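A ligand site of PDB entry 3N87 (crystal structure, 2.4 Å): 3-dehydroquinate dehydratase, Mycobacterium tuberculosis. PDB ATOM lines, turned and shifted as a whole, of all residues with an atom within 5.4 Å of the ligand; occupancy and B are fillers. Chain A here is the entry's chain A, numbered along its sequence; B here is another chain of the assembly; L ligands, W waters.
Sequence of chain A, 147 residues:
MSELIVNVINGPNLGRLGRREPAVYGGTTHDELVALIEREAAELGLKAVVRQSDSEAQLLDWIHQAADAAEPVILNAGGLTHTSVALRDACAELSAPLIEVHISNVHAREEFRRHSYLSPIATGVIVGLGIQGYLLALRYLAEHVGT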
ATOM      1  N   PRO A  12      10.401  30.134 -13.055  1.00  0.00           N
ATOM      2  CA  PRO A  12       9.819  29.093 -13.854  1.00  0.00           C
ATOM      3  C   PRO A  12       9.028  28.033 -13.111  1.00  0.00           C
ATOM      4  O   PRO A  12       9.461  27.557 -12.050  1.00  0.00           O
ATOM      5  CB  PRO A  12      11.043  28.459 -14.542  1.00  0.00           C
ATOM      6  CG  PRO A  12      11.988  29.588 -14.714  1.00  0.00           C
ATOM      7  CD  PRO A  12      11.777  30.455 -13.499  1.00  0.00           C
ATOM      8  N   ASN A  13       7.898  27.658 -13.704  1.00  0.00           N
ATOM      9  CA  ASN A  13       7.108  26.478 -13.285  1.00  0.00           C
ATOM     10  C   ASN A  13       6.227  26.727 -12.074  1.00  0.00           C
ATOM     11  O   ASN A  13       5.305  25.950 -11.794  1.00  0.00           O
ATOM     12  CB  ASN A  13       7.992  25.267 -13.018  1.00  0.00           C
ATOM     13  CG  ASN A  13       8.692  24.764 -14.256  1.00  0.00           C
ATOM     14  OD1 ASN A  13       8.086  24.670 -15.352  1.00  0.00           O
ATOM     15  ND2 ASN A  13       9.978  24.422 -14.093  1.00  0.00           N
ATOM     16  N   LEU A  14       6.554  27.800 -11.350  1.00  0.00           N
ATOM     17  CA  LEU A  14       5.908  28.147 -10.094  1.00  0.00           C
ATOM     18  C   LEU A  14       4.432  28.549 -10.275  1.00  0.00           C
ATOM     19  O   LEU A  14       3.653  28.478  -9.311  1.00  0.00           O
ATOM     20  CB  LEU A  14       6.693  29.255  -9.396  1.00  0.00           C
ATOM     21  CG  LEU A  14       7.872  28.750  -8.571  1.00  0.00           C
ATOM     22  CD1 LEU A  14       8.775  29.903  -8.127  1.00  0.00           C
ATOM     23  CD2 LEU A  14       7.398  27.918  -7.368  1.00  0.00           C
ATOM     24  N   ARG A  19      -0.682  21.617  -8.294  1.00  0.00           N
ATOM     25  CA  ARG A  19      -1.189  20.552  -9.197  1.00  0.00           C
ATOM     26  C   ARG A  19      -0.145  19.453  -9.601  1.00  0.00           C
ATOM     27  O   ARG A  19       0.306  19.392 -10.745  1.00  0.00           O
ATOM     28  CB  ARG A  19      -1.992  21.130 -10.390  1.00  0.00           C
ATOM     29  CG  ARG A  19      -1.289  22.114 -11.310  1.00  0.00           C
ATOM     30  CD  ARG A  19      -1.906  21.971 -12.696  1.00  0.00           C
ATOM     31  NE  ARG A  19      -1.798  23.145 -13.587  1.00  0.00           N
ATOM     32  CZ  ARG A  19      -2.448  24.301 -13.418  1.00  0.00           C
ATOM     33  NH1 ARG A  19      -3.237  24.504 -12.375  1.00  0.00           N
ATOM     34  NH2 ARG A  19      -2.291  25.289 -14.311  1.00  0.00           N
ATOM     35  N   ARG A  20       0.190  18.601  -8.625  1.00  0.00           N
ATOM     36  CA  ARG A  20       1.152  17.475  -8.737  1.00  0.00           C
ATOM     37  C   ARG A  20       2.050  17.568  -7.533  1.00  0.00           C
ATOM     38  O   ARG A  20       2.234  18.650  -6.990  1.00  0.00           O
ATOM     39  CB  ARG A  20       1.999  17.487 -10.023  1.00  0.00           C
ATOM     40  N   GLU A  21       2.610  16.423  -7.121  1.00  0.00           N
ATOM     41  CA  GLU A  21       3.512  16.327  -5.959  1.00  0.00           C
ATOM     42  C   GLU A  21       3.274  17.378  -4.870  1.00  0.00           C
ATOM     43  O   GLU A  21       4.161  18.194  -4.552  1.00  0.00           O
ATOM     44  CB  GLU A  21       4.963  16.392  -6.411  1.00  0.00           C
ATOM     45  CG  GLU A  21       5.643  15.078  -6.375  1.00  0.00           C
ATOM     46  CD  GLU A  21       6.860  15.090  -7.244  1.00  0.00           C
ATOM     47  OE1 GLU A  21       7.478  16.177  -7.396  1.00  0.00           O
ATOM     48  OE2 GLU A  21       7.190  14.010  -7.795  1.00  0.00           O
ATOM     49  N   TYR A  25       6.057  20.622  -2.670  1.00  0.00           N
ATOM     50  CA  TYR A  25       5.756  22.053  -2.880  1.00  0.00           C
ATOM     51  C   TYR A  25       4.398  22.375  -2.245  1.00  0.00           C
ATOM     52  O   TYR A  25       3.854  21.547  -1.522  1.00  0.00           O
ATOM     53  CB  TYR A  25       5.848  22.415  -4.366  1.00  0.00           C
ATOM     54  CG  TYR A  25       7.149  21.956  -4.999  1.00  0.00           C
ATOM     55  CD1 TYR A  25       7.270  20.668  -5.552  1.00  0.00           C
ATOM     56  CD2 TYR A  25       8.280  22.783  -5.007  1.00  0.00           C
ATOM     57  CE1 TYR A  25       8.461  20.229  -6.102  1.00  0.00           C
ATOM     58  CE2 TYR A  25       9.492  22.345  -5.564  1.00  0.00           C
ATOM     59  CZ  TYR A  25       9.570  21.064  -6.117  1.00  0.00           C
ATOM     60  OH  TYR A  25      10.758  20.622  -6.676  1.00  0.00           O
ATOM     61  N   ASN A  76      11.824  33.666  -5.423  1.00  0.00           N
ATOM     62  CA  ASN A  76      11.903  32.215  -5.547  1.00  0.00           C
ATOM     63  C   ASN A  76      12.108  31.920  -7.027  1.00  0.00           C
ATOM     64  O   ASN A  76      11.139  31.877  -7.804  1.00  0.00           O
ATOM     65  CB  ASN A  76      10.664  31.517  -4.974  1.00  0.00           C
ATOM     66  CG  ASN A  76      10.688  30.026  -5.198  1.00  0.00           C
ATOM     67  OD1 ASN A  76      11.541  29.517  -5.948  1.00  0.00           O
ATOM     68  ND2 ASN A  76       9.747  29.299  -4.564  1.00  0.00           N
ATOM     69  N   ALA A  77      13.365  31.737  -7.403  1.00  0.00           N
ATOM     70  CA  ALA A  77      13.750  31.774  -8.818  1.00  0.00           C
ATOM     71  C   ALA A  77      13.574  30.400  -9.466  1.00  0.00           C
ATOM     72  O   ALA A  77      13.822  30.233 -10.696  1.00  0.00           O
ATOM     73  CB  ALA A  77      15.219  32.322  -8.997  1.00  0.00           C
ATOM     74  N   GLY A  78      13.126  29.460  -8.622  1.00  0.00           N
ATOM     75  CA  GLY A  78      13.090  28.017  -8.900  1.00  0.00           C
ATOM     76  C   GLY A  78      14.284  27.625  -9.724  1.00  0.00           C
ATOM     77  O   GLY A  78      15.366  28.170  -9.501  1.00  0.00           O
ATOM     78  N   GLY A  79      14.083  26.750 -10.705  1.00  0.00           N
ATOM     79  CA  GLY A  79      15.151  26.294 -11.621  1.00  0.00           C
ATOM     80  C   GLY A  79      16.322  27.222 -11.891  1.00  0.00           C
ATOM     81  O   GLY A  79      17.467  26.791 -11.828  1.00  0.00           O
ATOM     82  N   THR A  81      17.636  29.296  -9.981  1.00  0.00           N
ATOM     83  CA  THR A  81      18.416  29.479  -8.773  1.00  0.00           C
ATOM     84  C   THR A  81      19.806  28.898  -8.977  1.00  0.00           C
ATOM     85  O   THR A  81      20.829  29.464  -8.577  1.00  0.00           O
ATOM     86  CB  THR A  81      17.699  28.805  -7.596  1.00  0.00           C
ATOM     87  OG1 THR A  81      16.376  29.352  -7.522  1.00  0.00           O
ATOM     88  CG2 THR A  81      18.435  29.088  -6.332  1.00  0.00           C
ATOM     89  N   HIS A  82      19.824  27.786  -9.685  1.00  0.00           N
ATOM     90  CA  HIS A  82      20.988  26.972  -9.809  1.00  0.00           C
ATOM     91  C   HIS A  82      21.785  27.286 -11.057  1.00  0.00           C
ATOM     92  O   HIS A  82      22.922  26.850 -11.157  1.00  0.00           O
ATOM     93  CB  HIS A  82      20.555  25.513  -9.812  1.00  0.00           C
ATOM     94  CG  HIS A  82      19.521  25.187  -8.774  1.00  0.00           C
ATOM     95  ND1 HIS A  82      19.769  25.288  -7.421  1.00  0.00           N
ATOM     96  CD2 HIS A  82      18.237  24.785  -8.896  1.00  0.00           C
ATOM     97  CE1 HIS A  82      18.686  24.947  -6.752  1.00  0.00           C
ATOM     98  NE2 HIS A  82      17.748  24.631  -7.616  1.00  0.00           N
ATOM     99  N   VAL A 101      13.917  32.762  -1.383  1.00  0.00           N
ATOM    100  CA  VAL A 101      13.032  31.787  -0.786  1.00  0.00           C
ATOM    101  C   VAL A 101      12.894  30.512  -1.607  1.00  0.00           C
ATOM    102  O   VAL A 101      12.769  30.551  -2.838  1.00  0.00           O
ATOM    103  CB  VAL A 101      11.643  32.417  -0.500  1.00  0.00           C
ATOM    104  CG1 VAL A 101      10.576  31.353  -0.147  1.00  0.00           C
ATOM    105  CG2 VAL A 101      11.769  33.422   0.635  1.00  0.00           C
ATOM    106  N   HIS A 102      12.928  29.385  -0.901  1.00  0.00           N
ATOM    107  CA  HIS A 102      12.527  28.132  -1.490  1.00  0.00           C
ATOM    108  C   HIS A 102      11.478  27.486  -0.629  1.00  0.00           C
ATOM    109  O   HIS A 102      11.561  27.516   0.601  1.00  0.00           O
ATOM    110  CB  HIS A 102      13.753  27.226  -1.700  1.00  0.00           C
ATOM    111  CG  HIS A 102      14.850  27.908  -2.456  1.00  0.00           C
ATOM    112  ND1 HIS A 102      14.864  28.011  -3.833  1.00  0.00           N
ATOM    113  CD2 HIS A 102      15.955  28.573  -2.029  1.00  0.00           C
ATOM    114  CE1 HIS A 102      15.925  28.697  -4.223  1.00  0.00           C
ATOM    115  NE2 HIS A 102      16.612  29.042  -3.145  1.00  0.00           N
ATOM    116  N   ILE A 103      10.460  26.924  -1.278  1.00  0.00           N
ATOM    117  CA  ILE A 103       9.432  26.194  -0.593  1.00  0.00           C
ATOM    118  C   ILE A 103       9.988  24.842  -0.137  1.00  0.00           C
ATOM    119  O   ILE A 103       9.801  24.451   1.024  1.00  0.00           O
ATOM    120  CB  ILE A 103       8.231  25.958  -1.492  1.00  0.00           C
ATOM    121  CG1 ILE A 103       7.627  27.300  -1.952  1.00  0.00           C
ATOM    122  CG2 ILE A 103       7.204  25.046  -0.797  1.00  0.00           C
ATOM    123  CD1 ILE A 103       6.856  27.162  -3.235  1.00  0.00           C
ATOM    124  N   SER A 104      10.646  24.113  -1.044  1.00  0.00           N
ATOM    125  CA  SER A 104      11.171  22.777  -0.673  1.00  0.00           C
ATOM    126  C   SER A 104      12.451  22.935   0.164  1.00  0.00           C
ATOM    127  O   SER A 104      13.019  24.014   0.197  1.00  0.00           O
ATOM    128  CB  SER A 104      11.421  21.894  -1.928  1.00  0.00           C
ATOM    129  OG  SER A 104      12.798  21.863  -2.342  1.00  0.00           O
ATOM    130  N   ASN A 105      12.893  21.882   0.846  1.00  0.00           N
ATOM    131  CA  ASN A 105      14.245  21.890   1.404  1.00  0.00           C
ATOM    132  C   ASN A 105      15.267  21.432   0.359  1.00  0.00           C
ATOM    133  O   ASN A 105      15.461  20.235   0.161  1.00  0.00           O
ATOM    134  CB  ASN A 105      14.298  21.015   2.645  1.00  0.00           C
ATOM    135  CG  ASN A 105      15.645  21.127   3.432  1.00  0.00           C
ATOM    136  OD1 ASN A 105      16.650  21.663   2.960  1.00  0.00           O
ATOM    137  ND2 ASN A 105      15.627  20.617   4.650  1.00  0.00           N
ATOM    138  N   VAL A 106      15.937  22.397  -0.288  1.00  0.00           N
ATOM    139  CA  VAL A 106      16.894  22.111  -1.354  1.00  0.00           C
ATOM    140  C   VAL A 106      18.130  21.324  -0.888  1.00  0.00           C
ATOM    141  O   VAL A 106      18.858  20.740  -1.716  1.00  0.00           O
ATOM    142  CB  VAL A 106      17.364  23.400  -2.023  1.00  0.00           C
ATOM    143  CG1 VAL A 106      16.130  24.153  -2.644  1.00  0.00           C
ATOM    144  CG2 VAL A 106      18.144  24.277  -1.026  1.00  0.00           C
ATOM    145  N   ARG A 109      17.531  17.242  -1.205  1.00  0.00           N
ATOM    146  CA  ARG A 109      17.254  16.684  -2.512  1.00  0.00           C
ATOM    147  C   ARG A 109      18.526  16.572  -3.397  1.00  0.00           C
ATOM    148  O   ARG A 109      19.627  16.510  -2.878  1.00  0.00           O
ATOM    149  CB  ARG A 109      16.204  17.564  -3.149  1.00  0.00           C
ATOM    150  CG  ARG A 109      15.049  17.903  -2.195  1.00  0.00           C
ATOM    151  CD  ARG A 109      14.098  18.900  -2.851  1.00  0.00           C
ATOM    152  NE  ARG A 109      13.681  18.471  -4.196  1.00  0.00           N
ATOM    153  CZ  ARG A 109      13.207  19.279  -5.144  1.00  0.00           C
ATOM    154  NH1 ARG A 109      13.082  20.588  -4.931  1.00  0.00           N
ATOM    155  NH2 ARG A 109      12.864  18.792  -6.324  1.00  0.00           N
ATOM    156  N   ARG A 113      20.756  20.852  -6.664  1.00  0.00           N
ATOM    157  CA  ARG A 113      19.892  21.830  -6.017  1.00  0.00           C
ATOM    158  C   ARG A 113      20.608  22.550  -4.864  1.00  0.00           C
ATOM    159  O   ARG A 113      20.116  23.586  -4.423  1.00  0.00           O
ATOM    160  CB  ARG A 113      18.568  21.227  -5.563  1.00  0.00           C
ATOM    161  CG  ARG A 113      17.831  20.442  -6.641  1.00  0.00           C
ATOM    162  CD  ARG A 113      16.329  20.322  -6.320  1.00  0.00           C
ATOM    163  NE  ARG A 113      15.617  19.537  -7.350  1.00  0.00           N
ATOM    164  CZ  ARG A 113      15.375  19.973  -8.580  1.00  0.00           C
ATOM    165  NH1 ARG A 113      15.778  21.188  -8.934  1.00  0.00           N
ATOM    166  NH2 ARG A 113      14.761  19.205  -9.459  1.00  0.00           N
ATOM    167  N   VAL B  85      17.826  23.555 -15.485  1.00  0.00           N
ATOM    168  CA  VAL B  85      16.982  22.899 -14.497  1.00  0.00           C
ATOM    169  C   VAL B  85      15.483  23.219 -14.717  1.00  0.00           C
ATOM    170  O   VAL B  85      14.626  22.340 -14.599  1.00  0.00           O
ATOM    171  CB  VAL B  85      17.459  23.232 -13.081  1.00  0.00           C
ATOM    172  CG1 VAL B  85      16.531  22.618 -12.081  1.00  0.00           C
ATOM    173  CG2 VAL B  85      18.875  22.706 -12.869  1.00  0.00           C
ATOM    174  N   ASP B  89      12.564  20.457 -14.740  1.00  0.00           N
ATOM    175  CA  ASP B  89      11.532  20.486 -13.723  1.00  0.00           C
ATOM    176  C   ASP B  89      10.148  20.476 -14.392  1.00  0.00           C
ATOM    177  O   ASP B  89       9.220  19.793 -13.945  1.00  0.00           O
ATOM    178  CB  ASP B  89      11.744  21.650 -12.751  1.00  0.00           C
ATOM    179  CG  ASP B  89      12.739  21.322 -11.611  1.00  0.00           C
ATOM    180  OD1 ASP B  89      12.864  20.156 -11.187  1.00  0.00           O
ATOM    181  OD2 ASP B  89      13.400  22.264 -11.112  1.00  0.00           O
ATOM    182  N   ALA B  90      10.047  21.189 -15.501  1.00  0.00           N
ATOM    183  CA  ALA B  90       8.831  21.084 -16.278  1.00  0.00           C
ATOM    184  C   ALA B  90       8.605  19.625 -16.757  1.00  0.00           C
ATOM    185  O   ALA B  90       7.516  19.091 -16.626  1.00  0.00           O
ATOM    186  CB  ALA B  90       8.878  22.031 -17.421  1.00  0.00           C
ATOM    187  N   ALA B  92       9.436  17.069 -15.266  1.00  0.00           N
ATOM    188  CA  ALA B  92       9.228  16.219 -14.118  1.00  0.00           C
ATOM    189  C   ALA B  92       7.756  15.965 -13.847  1.00  0.00           C
ATOM    190  O   ALA B  92       7.381  14.942 -13.249  1.00  0.00           O
ATOM    191  CB  ALA B  92       9.881  16.839 -12.931  1.00  0.00           C
ATOM    192  N   GLU B  93       6.917  16.902 -14.271  1.00  0.00           N
ATOM    193  CA  GLU B  93       5.475  16.852 -14.095  1.00  0.00           C
ATOM    194  C   GLU B  93       4.830  15.737 -14.925  1.00  0.00           C
ATOM    195  O   GLU B  93       3.856  15.144 -14.485  1.00  0.00           O
ATOM    196  CB  GLU B  93       4.862  18.167 -14.530  1.00  0.00           C
ATOM    197  CG  GLU B  93       4.226  19.046 -13.463  1.00  0.00           C
ATOM    198  CD  GLU B  93       3.624  20.314 -14.096  1.00  0.00           C
ATOM    199  OE1 GLU B  93       2.368  20.490 -14.107  1.00  0.00           O
ATOM    200  OE2 GLU B  93       4.411  21.132 -14.625  1.00  0.00           O
HETATM  201  O1  LIG L   1      10.899  26.636  -4.080  1.00  0.00           O
HETATM  202  C1  LIG L   1      11.635  25.646  -4.282  1.00  0.00           C
HETATM  203  O2  LIG L   1      11.691  24.686  -3.467  1.00  0.00           O
HETATM  204  C2  LIG L   1      12.437  25.661  -5.576  1.00  0.00           C
HETATM  205  O3  LIG L   1      12.952  26.980  -5.749  1.00  0.00           O
HETATM  206  C3  LIG L   1      11.516  25.482  -6.753  1.00  0.00           C
HETATM  207  C4  LIG L   1      11.687  24.584  -7.744  1.00  0.00           C
HETATM  208  C5  LIG L   1      13.021  23.937  -7.961  1.00  0.00           C
HETATM  209  O4  LIG L   1      13.367  24.189  -9.321  1.00  0.00           O
HETATM  210  C6  LIG L   1      14.088  24.501  -7.029  1.00  0.00           C
HETATM  211  O5  LIG L   1      15.243  23.663  -7.031  1.00  0.00           O
HETATM  212  C7  LIG L   1      13.561  24.626  -5.596  1.00  0.00           C
HETATM  213  C8  LIG L   1      10.472  24.216  -8.557  1.00  0.00           C
HETATM  214  C9  LIG L   1      10.254  22.885  -8.875  1.00  0.00           C
HETATM  215  C10 LIG L   1       9.145  22.480  -9.608  1.00  0.00           C
HETATM  216  C11 LIG L   1       9.032  21.001  -9.927  1.00  0.00           C
HETATM  217  C12 LIG L   1       7.784  20.163  -9.933  1.00  0.00           C
HETATM  218  C13 LIG L   1       6.502  20.710  -9.806  1.00  0.00           C
HETATM  219  C14 LIG L   1       5.401  19.859  -9.843  1.00  0.00           C
HETATM  220  C15 LIG L   1       5.586  18.478 -10.003  1.00  0.00           C
HETATM  221  C16 LIG L   1       6.865  17.927 -10.139  1.00  0.00           C
HETATM  222  C17 LIG L   1       7.959  18.773 -10.098  1.00  0.00           C
HETATM  223  C18 LIG L   1       8.212  23.450 -10.025  1.00  0.00           C
HETATM  224  C19 LIG L   1       8.400  24.798  -9.693  1.00  0.00           C
HETATM  225  C20 LIG L   1       9.534  25.184  -8.961  1.00  0.00           C
HETATM  226  O6  LIG L   1      10.050  20.417 -10.223  1.00  0.00           O
HETATM  227  O   HOH W   1      12.061  25.426 -11.588  1.00  0.00           O
HETATM  228  O   HOH W   2      11.414  17.733  -9.966  1.00  0.00           O
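O3 of the ligand lies within hydrogen-bond range of ND1 of His 102 (2.9 Å). A ring nitrogen (NE2) of His 82 is in hydrogen-bond range of an oxygen (O5) of the ligand (2.7 Å). The side-chain carboxylate of Asp 89 of chain B lies within hydrogen-bond range of an oxygen (O4) of the ligand, at 2.6 Å. OD1 of Asn 76 is in hydrogen-bond range of O3 of the ligand. The side-chain hydroxyl (OG) of Ser 104 sits close to an oxygen (O2) of the ligand (3.2 Å). O5 of the ligand lies within hydrogen-bond range of NH1 of Arg 113 (3.2 Å). The backbone NH (N) of Ile 103 is in hydrogen-bond range of an oxygen (O1) of the ligand (2.9 Å). An oxygen (O2) of the ligand is in hydrogen-bond range of the backbone NH (N) of Ser 104. An oxygen (O4) of the ligand sits at hydrogen-bond distance from the backbone NH of Gly 79, 3.0 Å away.
OG of Ser 104 is in hydrogen-bond range of NH1 of Arg 109, 2.9 Å away. O of Gly 78 sits at hydrogen-bond distance from OG1 of Thr 81 (2.5 Å). The side-chain hydroxyl (OH) of Tyr 25 is in hydrogen-bond range of the guanidinium group (NH2) of Arg 109, at 2.8 Å. OD1 of Asn 76 lies close to N of Gly 78 (3.1 Å). OD1 of Asn 76 sits close to O of Val 101, 3.5 Å away. ND1 of His 82 lies close to O of Arg 113. The side-chain carboxylate (OD1) of Asp 89 of chain B is in salt-bridge range of the guanidinium group (NH2) of Arg 113, at 2.7 Å.
Merely in contact with the ligand: Tyr 25 (3.2 Å), Glu 21 (3.3 Å), Gly 78 (3.3 Å), Asn 13 (3.4 Å), Arg 20 (3.7 Å), Glu 93 of chain B (3.8 Å), Pro 12 (3.8 Å), Leu 14 (3.8 Å), Ala 92 of chain B (3.9 Å) and Val 106 (3.9 Å). Of the 26 residues printed, 18 come within 4 Å of the ligand.
Water W1 lies within hydrogen-bond range of the backbone NH of Gly 79 (2.6 Å), an oxygen (O4) of the ligand (2.9 Å), the backbone carbonyl oxygen of Pro 12 (3.4 Å), the side-chain amide nitrogen of Asn 13 (3.4 Å) and the side-chain carboxylate of Asp 89 of chain B (3.5 Å). Water W2 bridges an oxygen (O6) of the ligand (3.0 Å) and the side-chain carboxylate (OD1) of Asp 89 of chain B (3.1 Å).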
